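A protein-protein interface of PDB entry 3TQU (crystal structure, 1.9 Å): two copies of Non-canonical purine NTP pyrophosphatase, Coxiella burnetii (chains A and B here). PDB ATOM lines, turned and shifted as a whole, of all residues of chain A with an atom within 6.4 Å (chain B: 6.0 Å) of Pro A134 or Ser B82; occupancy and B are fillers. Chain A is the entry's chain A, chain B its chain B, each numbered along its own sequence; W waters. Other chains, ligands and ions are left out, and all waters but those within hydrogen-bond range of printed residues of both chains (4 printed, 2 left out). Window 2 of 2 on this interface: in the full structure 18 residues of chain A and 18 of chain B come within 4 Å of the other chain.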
ATOM      1  N   MET A 128      32.517  33.873  14.450  1.00  0.00           N
ATOM      2  CA  MET A 128      32.072  32.572  13.952  1.00  0.00           C
ATOM      3  C   MET A 128      33.263  31.667  13.657  1.00  0.00           C
ATOM      4  O   MET A 128      34.231  32.101  13.040  1.00  0.00           O
ATOM      5  CB  MET A 128      31.262  32.753  12.667  1.00  0.00           C
ATOM      6  CG  MET A 128      30.032  33.628  12.811  1.00  0.00           C
ATOM      7  SD  MET A 128      28.433  32.579  13.151  1.00  0.00           S
ATOM      8  CE  MET A 128      28.227  31.756  11.391  1.00  0.00           C
ATOM      9  N   ASN A 130      33.027  28.979  11.734  1.00  0.00           N
ATOM     10  CA  ASN A 130      32.830  28.907  10.289  1.00  0.00           C
ATOM     11  C   ASN A 130      31.400  29.300   9.939  1.00  0.00           C
ATOM     12  O   ASN A 130      30.628  29.672  10.822  1.00  0.00           O
ATOM     13  CB  ASN A 130      33.198  27.530   9.725  1.00  0.00           C
ATOM     14  CG  ASN A 130      32.409  26.400  10.357  1.00  0.00           C
ATOM     15  OD1 ASN A 130      31.195  26.494  10.540  1.00  0.00           O
ATOM     16  ND2 ASN A 130      33.101  25.319  10.693  1.00  0.00           N
ATOM     17  N   GLU A 131      31.041  29.230   8.662  1.00  0.00           N
ATOM     18  CA  GLU A 131      29.741  29.750   8.243  1.00  0.00           C
ATOM     19  C   GLU A 131      28.567  28.948   8.802  1.00  0.00           C
ATOM     20  O   GLU A 131      27.444  29.447   8.861  1.00  0.00           O
ATOM     21  CB  GLU A 131      29.641  29.870   6.716  1.00  0.00           C
ATOM     22  CG  GLU A 131      29.555  28.552   5.974  1.00  0.00           C
ATOM     23  CD  GLU A 131      30.917  28.005   5.608  1.00  0.00           C
ATOM     24  OE1 GLU A 131      31.894  28.298   6.329  1.00  0.00           O
ATOM     25  OE2 GLU A 131      31.011  27.286   4.592  1.00  0.00           O
ATOM     26  N   ASN A 132      28.829  27.714   9.222  1.00  0.00           N
ATOM     27  CA  ASN A 132      27.784  26.865   9.784  1.00  0.00           C
ATOM     28  C   ASN A 132      27.717  26.893  11.313  1.00  0.00           C
ATOM     29  O   ASN A 132      26.873  26.223  11.909  1.00  0.00           O
ATOM     30  CB  ASN A 132      27.928  25.420   9.292  1.00  0.00           C
ATOM     31  CG  ASN A 132      27.779  25.298   7.788  1.00  0.00           C
ATOM     32  OD1 ASN A 132      28.709  24.892   7.094  1.00  0.00           O
ATOM     33  ND2 ASN A 132      26.602  25.646   7.276  1.00  0.00           N
ATOM     34  N   ASP A 133      28.601  27.667  11.941  1.00  0.00           N
ATOM     35  CA  ASP A 133      28.611  27.805  13.397  1.00  0.00           C
ATOM     36  C   ASP A 133      27.262  28.324  13.903  1.00  0.00           C
ATOM     37  O   ASP A 133      26.852  29.433  13.559  1.00  0.00           O
ATOM     38  CB  ASP A 133      29.734  28.755  13.831  1.00  0.00           C
ATOM     39  CG  ASP A 133      29.946  28.777  15.342  1.00  0.00           C
ATOM     40  OD1 ASP A 133      29.129  28.195  16.085  1.00  0.00           O
ATOM     41  OD2 ASP A 133      30.937  29.390  15.785  1.00  0.00           O
ATOM     42  N   PRO A 134      26.564  27.515  14.717  1.00  0.00           N
ATOM     43  CA  PRO A 134      25.250  27.890  15.247  1.00  0.00           C
ATOM     44  C   PRO A 134      25.351  28.641  16.572  1.00  0.00           C
ATOM     45  O   PRO A 134      24.338  29.151  17.061  1.00  0.00           O
ATOM     46  CB  PRO A 134      24.587  26.535  15.477  1.00  0.00           C
ATOM     47  CG  PRO A 134      25.729  25.656  15.870  1.00  0.00           C
ATOM     48  CD  PRO A 134      26.914  26.123  15.055  1.00  0.00           C
ATOM     49  N   ALA A 135      26.553  28.703  17.138  1.00  0.00           N
ATOM     50  CA  ALA A 135      26.752  29.291  18.457  1.00  0.00           C
ATOM     51  C   ALA A 135      27.959  30.223  18.476  1.00  0.00           C
ATOM     52  O   ALA A 135      28.931  29.983  19.203  1.00  0.00           O
ATOM     53  CB  ALA A 135      26.912  28.200  19.499  1.00  0.00           C
ATOM     54  N   PRO A 136      27.903  31.292  17.671  1.00  0.00           N
ATOM     55  CA  PRO A 136      29.015  32.241  17.612  1.00  0.00           C
ATOM     56  C   PRO A 136      29.228  32.905  18.964  1.00  0.00           C
ATOM     57  O   PRO A 136      28.284  33.031  19.746  1.00  0.00           O
ATOM     58  CB  PRO A 136      28.534  33.279  16.591  1.00  0.00           C
ATOM     59  CG  PRO A 136      27.043  33.184  16.628  1.00  0.00           C
ATOM     60  CD  PRO A 136      26.758  31.730  16.852  1.00  0.00           C
ATOM     61  N   SER B  47      20.302  30.254  11.289  1.00  0.00           N
ATOM     62  CA  SER B  47      21.335  29.228  11.296  1.00  0.00           C
ATOM     63  C   SER B  47      22.066  29.248  12.635  1.00  0.00           C
ATOM     64  O   SER B  47      23.006  28.486  12.853  1.00  0.00           O
ATOM     65  CB  SER B  47      22.320  29.429  10.140  1.00  0.00           C
ATOM     66  OG  SER B  47      23.127  30.577  10.338  1.00  0.00           O
ATOM     67  N   THR B  48      21.629  30.131  13.530  1.00  0.00           N
ATOM     68  CA  THR B  48      22.193  30.207  14.876  1.00  0.00           C
ATOM     69  C   THR B  48      21.077  30.226  15.916  1.00  0.00           C
ATOM     70  O   THR B  48      19.964  30.670  15.633  1.00  0.00           O
ATOM     71  CB  THR B  48      23.068  31.464  15.060  1.00  0.00           C
ATOM     72  OG1 THR B  48      22.256  32.640  14.937  1.00  0.00           O
ATOM     73  CG2 THR B  48      24.186  31.504  14.021  1.00  0.00           C
ATOM     74  N   PHE B  49      21.376  29.740  17.119  1.00  0.00           N
ATOM     75  CA  PHE B  49      20.398  29.751  18.199  1.00  0.00           C
ATOM     76  C   PHE B  49      19.928  31.171  18.491  1.00  0.00           C
ATOM     77  O   PHE B  49      18.740  31.410  18.717  1.00  0.00           O
ATOM     78  CB  PHE B  49      20.983  29.131  19.473  1.00  0.00           C
ATOM     79  CG  PHE B  49      21.535  27.748  19.279  1.00  0.00           C
ATOM     80  CD1 PHE B  49      20.711  26.707  18.881  1.00  0.00           C
ATOM     81  CD2 PHE B  49      22.875  27.485  19.508  1.00  0.00           C
ATOM     82  CE1 PHE B  49      21.217  25.428  18.704  1.00  0.00           C
ATOM     83  CE2 PHE B  49      23.387  26.210  19.337  1.00  0.00           C
ATOM     84  CZ  PHE B  49      22.555  25.181  18.934  1.00  0.00           C
ATOM     85  N   VAL B  50      20.863  32.116  18.483  1.00  0.00           N
ATOM     86  CA  VAL B  50      20.538  33.500  18.798  1.00  0.00           C
ATOM     87  C   VAL B  50      19.546  34.063  17.783  1.00  0.00           C
ATOM     88  O   VAL B  50      18.561  34.701  18.157  1.00  0.00           O
ATOM     89  CB  VAL B  50      21.810  34.389  18.893  1.00  0.00           C
ATOM     90  CG1 VAL B  50      22.596  34.343  17.603  1.00  0.00           C
ATOM     91  CG2 VAL B  50      21.438  35.821  19.258  1.00  0.00           C
ATOM     92  N   LEU B  75      22.361  20.847  20.479  1.00  0.00           N
ATOM     93  CA  LEU B  75      23.578  20.114  20.773  1.00  0.00           C
ATOM     94  C   LEU B  75      24.530  20.300  19.609  1.00  0.00           C
ATOM     95  O   LEU B  75      24.133  20.118  18.462  1.00  0.00           O
ATOM     96  CB  LEU B  75      23.256  18.628  20.917  1.00  0.00           C
ATOM     97  CG  LEU B  75      24.438  17.663  21.042  1.00  0.00           C
ATOM     98  CD1 LEU B  75      25.219  17.930  22.322  1.00  0.00           C
ATOM     99  CD2 LEU B  75      23.952  16.224  21.000  1.00  0.00           C
ATOM    100  N   THR B  76      25.775  20.666  19.899  1.00  0.00           N
ATOM    101  CA  THR B  76      26.792  20.804  18.860  1.00  0.00           C
ATOM    102  C   THR B  76      27.880  19.756  19.059  1.00  0.00           C
ATOM    103  O   THR B  76      28.427  19.615  20.150  1.00  0.00           O
ATOM    104  CB  THR B  76      27.436  22.219  18.832  1.00  0.00           C
ATOM    105  OG1 THR B  76      28.120  22.474  20.065  1.00  0.00           O
ATOM    106  CG2 THR B  76      26.383  23.295  18.606  1.00  0.00           C
ATOM    107  N   ILE B  77      28.185  19.019  17.997  1.00  0.00           N
ATOM    108  CA  ILE B  77      29.180  17.958  18.064  1.00  0.00           C
ATOM    109  C   ILE B  77      30.365  18.274  17.152  1.00  0.00           C
ATOM    110  O   ILE B  77      30.207  18.438  15.939  1.00  0.00           O
ATOM    111  CB  ILE B  77      28.564  16.597  17.696  1.00  0.00           C
ATOM    112  CG1 ILE B  77      27.388  16.295  18.628  1.00  0.00           C
ATOM    113  CG2 ILE B  77      29.619  15.494  17.756  1.00  0.00           C
ATOM    114  CD1 ILE B  77      26.564  15.085  18.234  1.00  0.00           C
ATOM    115  N   ALA B  78      31.551  18.356  17.748  1.00  0.00           N
ATOM    116  CA  ALA B  78      32.744  18.809  17.039  1.00  0.00           C
ATOM    117  C   ALA B  78      33.062  17.984  15.792  1.00  0.00           C
ATOM    118  O   ALA B  78      33.371  18.540  14.739  1.00  0.00           O
ATOM    119  CB  ALA B  78      33.947  18.840  17.984  1.00  0.00           C
ATOM    120  N   ALA B  79      32.984  16.662  15.914  1.00  0.00           N
ATOM    121  CA  ALA B  79      33.301  15.770  14.801  1.00  0.00           C
ATOM    122  C   ALA B  79      32.290  15.885  13.662  1.00  0.00           C
ATOM    123  O   ALA B  79      32.554  15.445  12.543  1.00  0.00           O
ATOM    124  CB  ALA B  79      33.396  14.324  15.285  1.00  0.00           C
ATOM    125  N   LEU B  80      31.133  16.474  13.952  1.00  0.00           N
ATOM    126  CA  LEU B  80      30.092  16.644  12.944  1.00  0.00           C
ATOM    127  C   LEU B  80      29.948  18.111  12.544  1.00  0.00           C
ATOM    128  O   LEU B  80      28.908  18.525  12.031  1.00  0.00           O
ATOM    129  CB  LEU B  80      28.755  16.104  13.454  1.00  0.00           C
ATOM    130  CG  LEU B  80      28.741  14.645  13.914  1.00  0.00           C
ATOM    131  CD1 LEU B  80      27.340  14.228  14.341  1.00  0.00           C
ATOM    132  CD2 LEU B  80      29.257  13.735  12.814  1.00  0.00           C
ATOM    133  N   ASN B  81      31.000  18.888  12.783  1.00  0.00           N
ATOM    134  CA  ASN B  81      31.004  20.311  12.455  1.00  0.00           C
ATOM    135  C   ASN B  81      29.865  21.054  13.150  1.00  0.00           C
ATOM    136  O   ASN B  81      29.154  21.846  12.529  1.00  0.00           O
ATOM    137  CB  ASN B  81      30.937  20.518  10.938  1.00  0.00           C
ATOM    138  CG  ASN B  81      31.325  21.926  10.520  1.00  0.00           C
ATOM    139  OD1 ASN B  81      32.115  22.589  11.190  1.00  0.00           O
ATOM    140  ND2 ASN B  81      30.766  22.388   9.408  1.00  0.00           N
ATOM    141  N   SER B  82      29.699  20.773  14.440  1.00  0.00           N
ATOM    142  CA  SER B  82      28.709  21.437  15.293  1.00  0.00           C
ATOM    143  C   SER B  82      27.261  20.996  15.060  1.00  0.00           C
ATOM    144  O   SER B  82      26.340  21.516  15.687  1.00  0.00           O
ATOM    145  CB  SER B  82      28.840  22.963  15.217  1.00  0.00           C
ATOM    146  OG  SER B  82      29.942  23.409  15.994  1.00  0.00           O
ATOM    147  N   ALA B  83      27.062  20.034  14.165  1.00  0.00           N
ATOM    148  CA  ALA B  83      25.743  19.435  13.985  1.00  0.00           C
ATOM    149  C   ALA B  83      25.410  18.578  15.210  1.00  0.00           C
ATOM    150  O   ALA B  83      26.318  18.108  15.897  1.00  0.00           O
ATOM    151  CB  ALA B  83      25.716  18.599  12.717  1.00  0.00           C
ATOM    152  N   PRO B  84      24.110  18.369  15.496  1.00  0.00           N
ATOM    153  CA  PRO B  84      22.923  18.831  14.762  1.00  0.00           C
ATOM    154  C   PRO B  84      22.665  20.335  14.843  1.00  0.00           C
ATOM    155  O   PRO B  84      21.956  20.860  13.989  1.00  0.00           O
ATOM    156  CB  PRO B  84      21.776  18.075  15.444  1.00  0.00           C
ATOM    157  CG  PRO B  84      22.277  17.786  16.810  1.00  0.00           C
ATOM    158  CD  PRO B  84      23.744  17.516  16.640  1.00  0.00           C
ATOM    159  N   GLY B  85      23.206  21.006  15.857  1.00  0.00           N
ATOM    160  CA  GLY B  85      23.099  22.454  15.958  1.00  0.00           C
ATOM    161  C   GLY B  85      21.678  22.994  15.980  1.00  0.00           C
ATOM    162  O   GLY B  85      20.873  22.595  16.820  1.00  0.00           O
ATOM    163  N   VAL B  86      21.371  23.914  15.068  1.00  0.00           N
ATOM    164  CA  VAL B  86      20.030  24.498  15.007  1.00  0.00           C
ATOM    165  C   VAL B  86      19.003  23.508  14.479  1.00  0.00           C
ATOM    166  O   VAL B  86      17.799  23.761  14.530  1.00  0.00           O
ATOM    167  CB  VAL B  86      19.978  25.786  14.152  1.00  0.00           C
ATOM    168  CG1 VAL B  86      20.666  26.926  14.874  1.00  0.00           C
ATOM    169  CG2 VAL B  86      20.590  25.549  12.778  1.00  0.00           C
ATOM    170  N   VAL B 124      20.533  29.740  24.282  1.00  0.00           N
ATOM    171  CA  VAL B 124      20.595  31.178  24.084  1.00  0.00           C
ATOM    172  C   VAL B 124      19.237  31.794  24.368  1.00  0.00           C
ATOM    173  O   VAL B 124      18.234  31.420  23.757  1.00  0.00           O
ATOM    174  CB  VAL B 124      21.031  31.546  22.661  1.00  0.00           C
ATOM    175  CG1 VAL B 124      21.049  33.064  22.494  1.00  0.00           C
ATOM    176  CG2 VAL B 124      22.397  30.953  22.349  1.00  0.00           C
HETATM  177  O   HOH W   1      25.555  29.511  11.011  1.00  0.00           O
HETATM  178  O   HOH W   2      23.687  31.464  18.665  1.00  0.00           O
HETATM  179  O   HOH W   3      33.658  23.307  13.267  1.00  0.00           O
HETATM  180  O   HOH W   4      24.058  26.276  11.576  1.00  0.00           O
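The side-chain amide nitrogen (ND2) of Asn A130 sits at hydrogen-bond distance from the side-chain amide oxygen (OD1) of Asn B81, 2.9 Å away.
The backbone NH of Phe B49 is in hydrogen-bond range of the backbone carbonyl oxygen of Pro A134.
N of Asn A132 sits at hydrogen-bond distance from OD1 of Asn A130, 3.0 Å away.
The side-chain amide oxygen of Asn A130 lies within hydrogen-bond range of the backbone NH of Asp A133 (3.2 Å).
The backbone NH (N) of Ala A135 sits at hydrogen-bond distance from the side-chain carboxylate (OD1) of Asp A133 (2.8 Å).
The backbone carbonyl oxygen of Ile B77 is in hydrogen-bond range of the backbone NH of Ser B82, at 2.8 Å.
Among the printed residues, merely in contact across the chains: Pro A134 with Thr B48, Pro A134 with Ser B47, Asp A133 with Thr B48, Pro A134 with Thr B76, Pro A134 with Ser B82, Pro A136 with Thr B48, Asn A132 with Asn B81 and Pro A134 with Val B86.
Of the printed residues of chain B, Pro A134 touches Ser B47 (3.3 Å), Thr B48 (3.2 Å), Phe B49 (3.0 Å), Thr B76 (3.7 Å), Ser B82 (3.7 Å) and Val B86 (3.99 Å).
Of the printed residues of chain A, Ser B47 touches Pro A134.
Printed residues of chain A within 4 Å of Thr B48: Asp A133, Pro A134 and Pro A136.
Ser B82 touches just one residue of chain A: Pro A134.
The nearest printed residue of chain A that does not touch Thr B76 is Ala A135 (5.0 Å).
Of the 8 printed residues of chain A, 5 touch a printed residue of chain B.
Hydrophobic or aromatic side chains of chain B within 4 Å of the printed part of chain A: Phe B49 and Val B86.
Among the printed residues, 10 pairs touch across the chains.
Among the printed residues, no Asp or Glu carboxylate lies within 4 Å of a Lys or Arg side-chain nitrogen of the other chain.
No position is printed for both chains.
Of the 10 pairs that touch across the chains among the printed residues, none has its exchanged pair printed and touching as well.
Water W3 lies within hydrogen-bond range of the side-chain amide oxygen of Asn B81 and the side-chain amide nitrogen of Asn A130.
Water W1 lies within hydrogen-bond range of OG of Ser B47 (2.7 Å), O of Asp A133 (2.9 Å) and O of Glu A131 (2.9 Å).
Water W4 bridges the backbone carbonyl oxygen of Ser B47 and the backbone carbonyl oxygen of Asn A132.
Water W2 lies within hydrogen-bond range of O of Pro A134, N of Val B50 and N of Phe B49.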
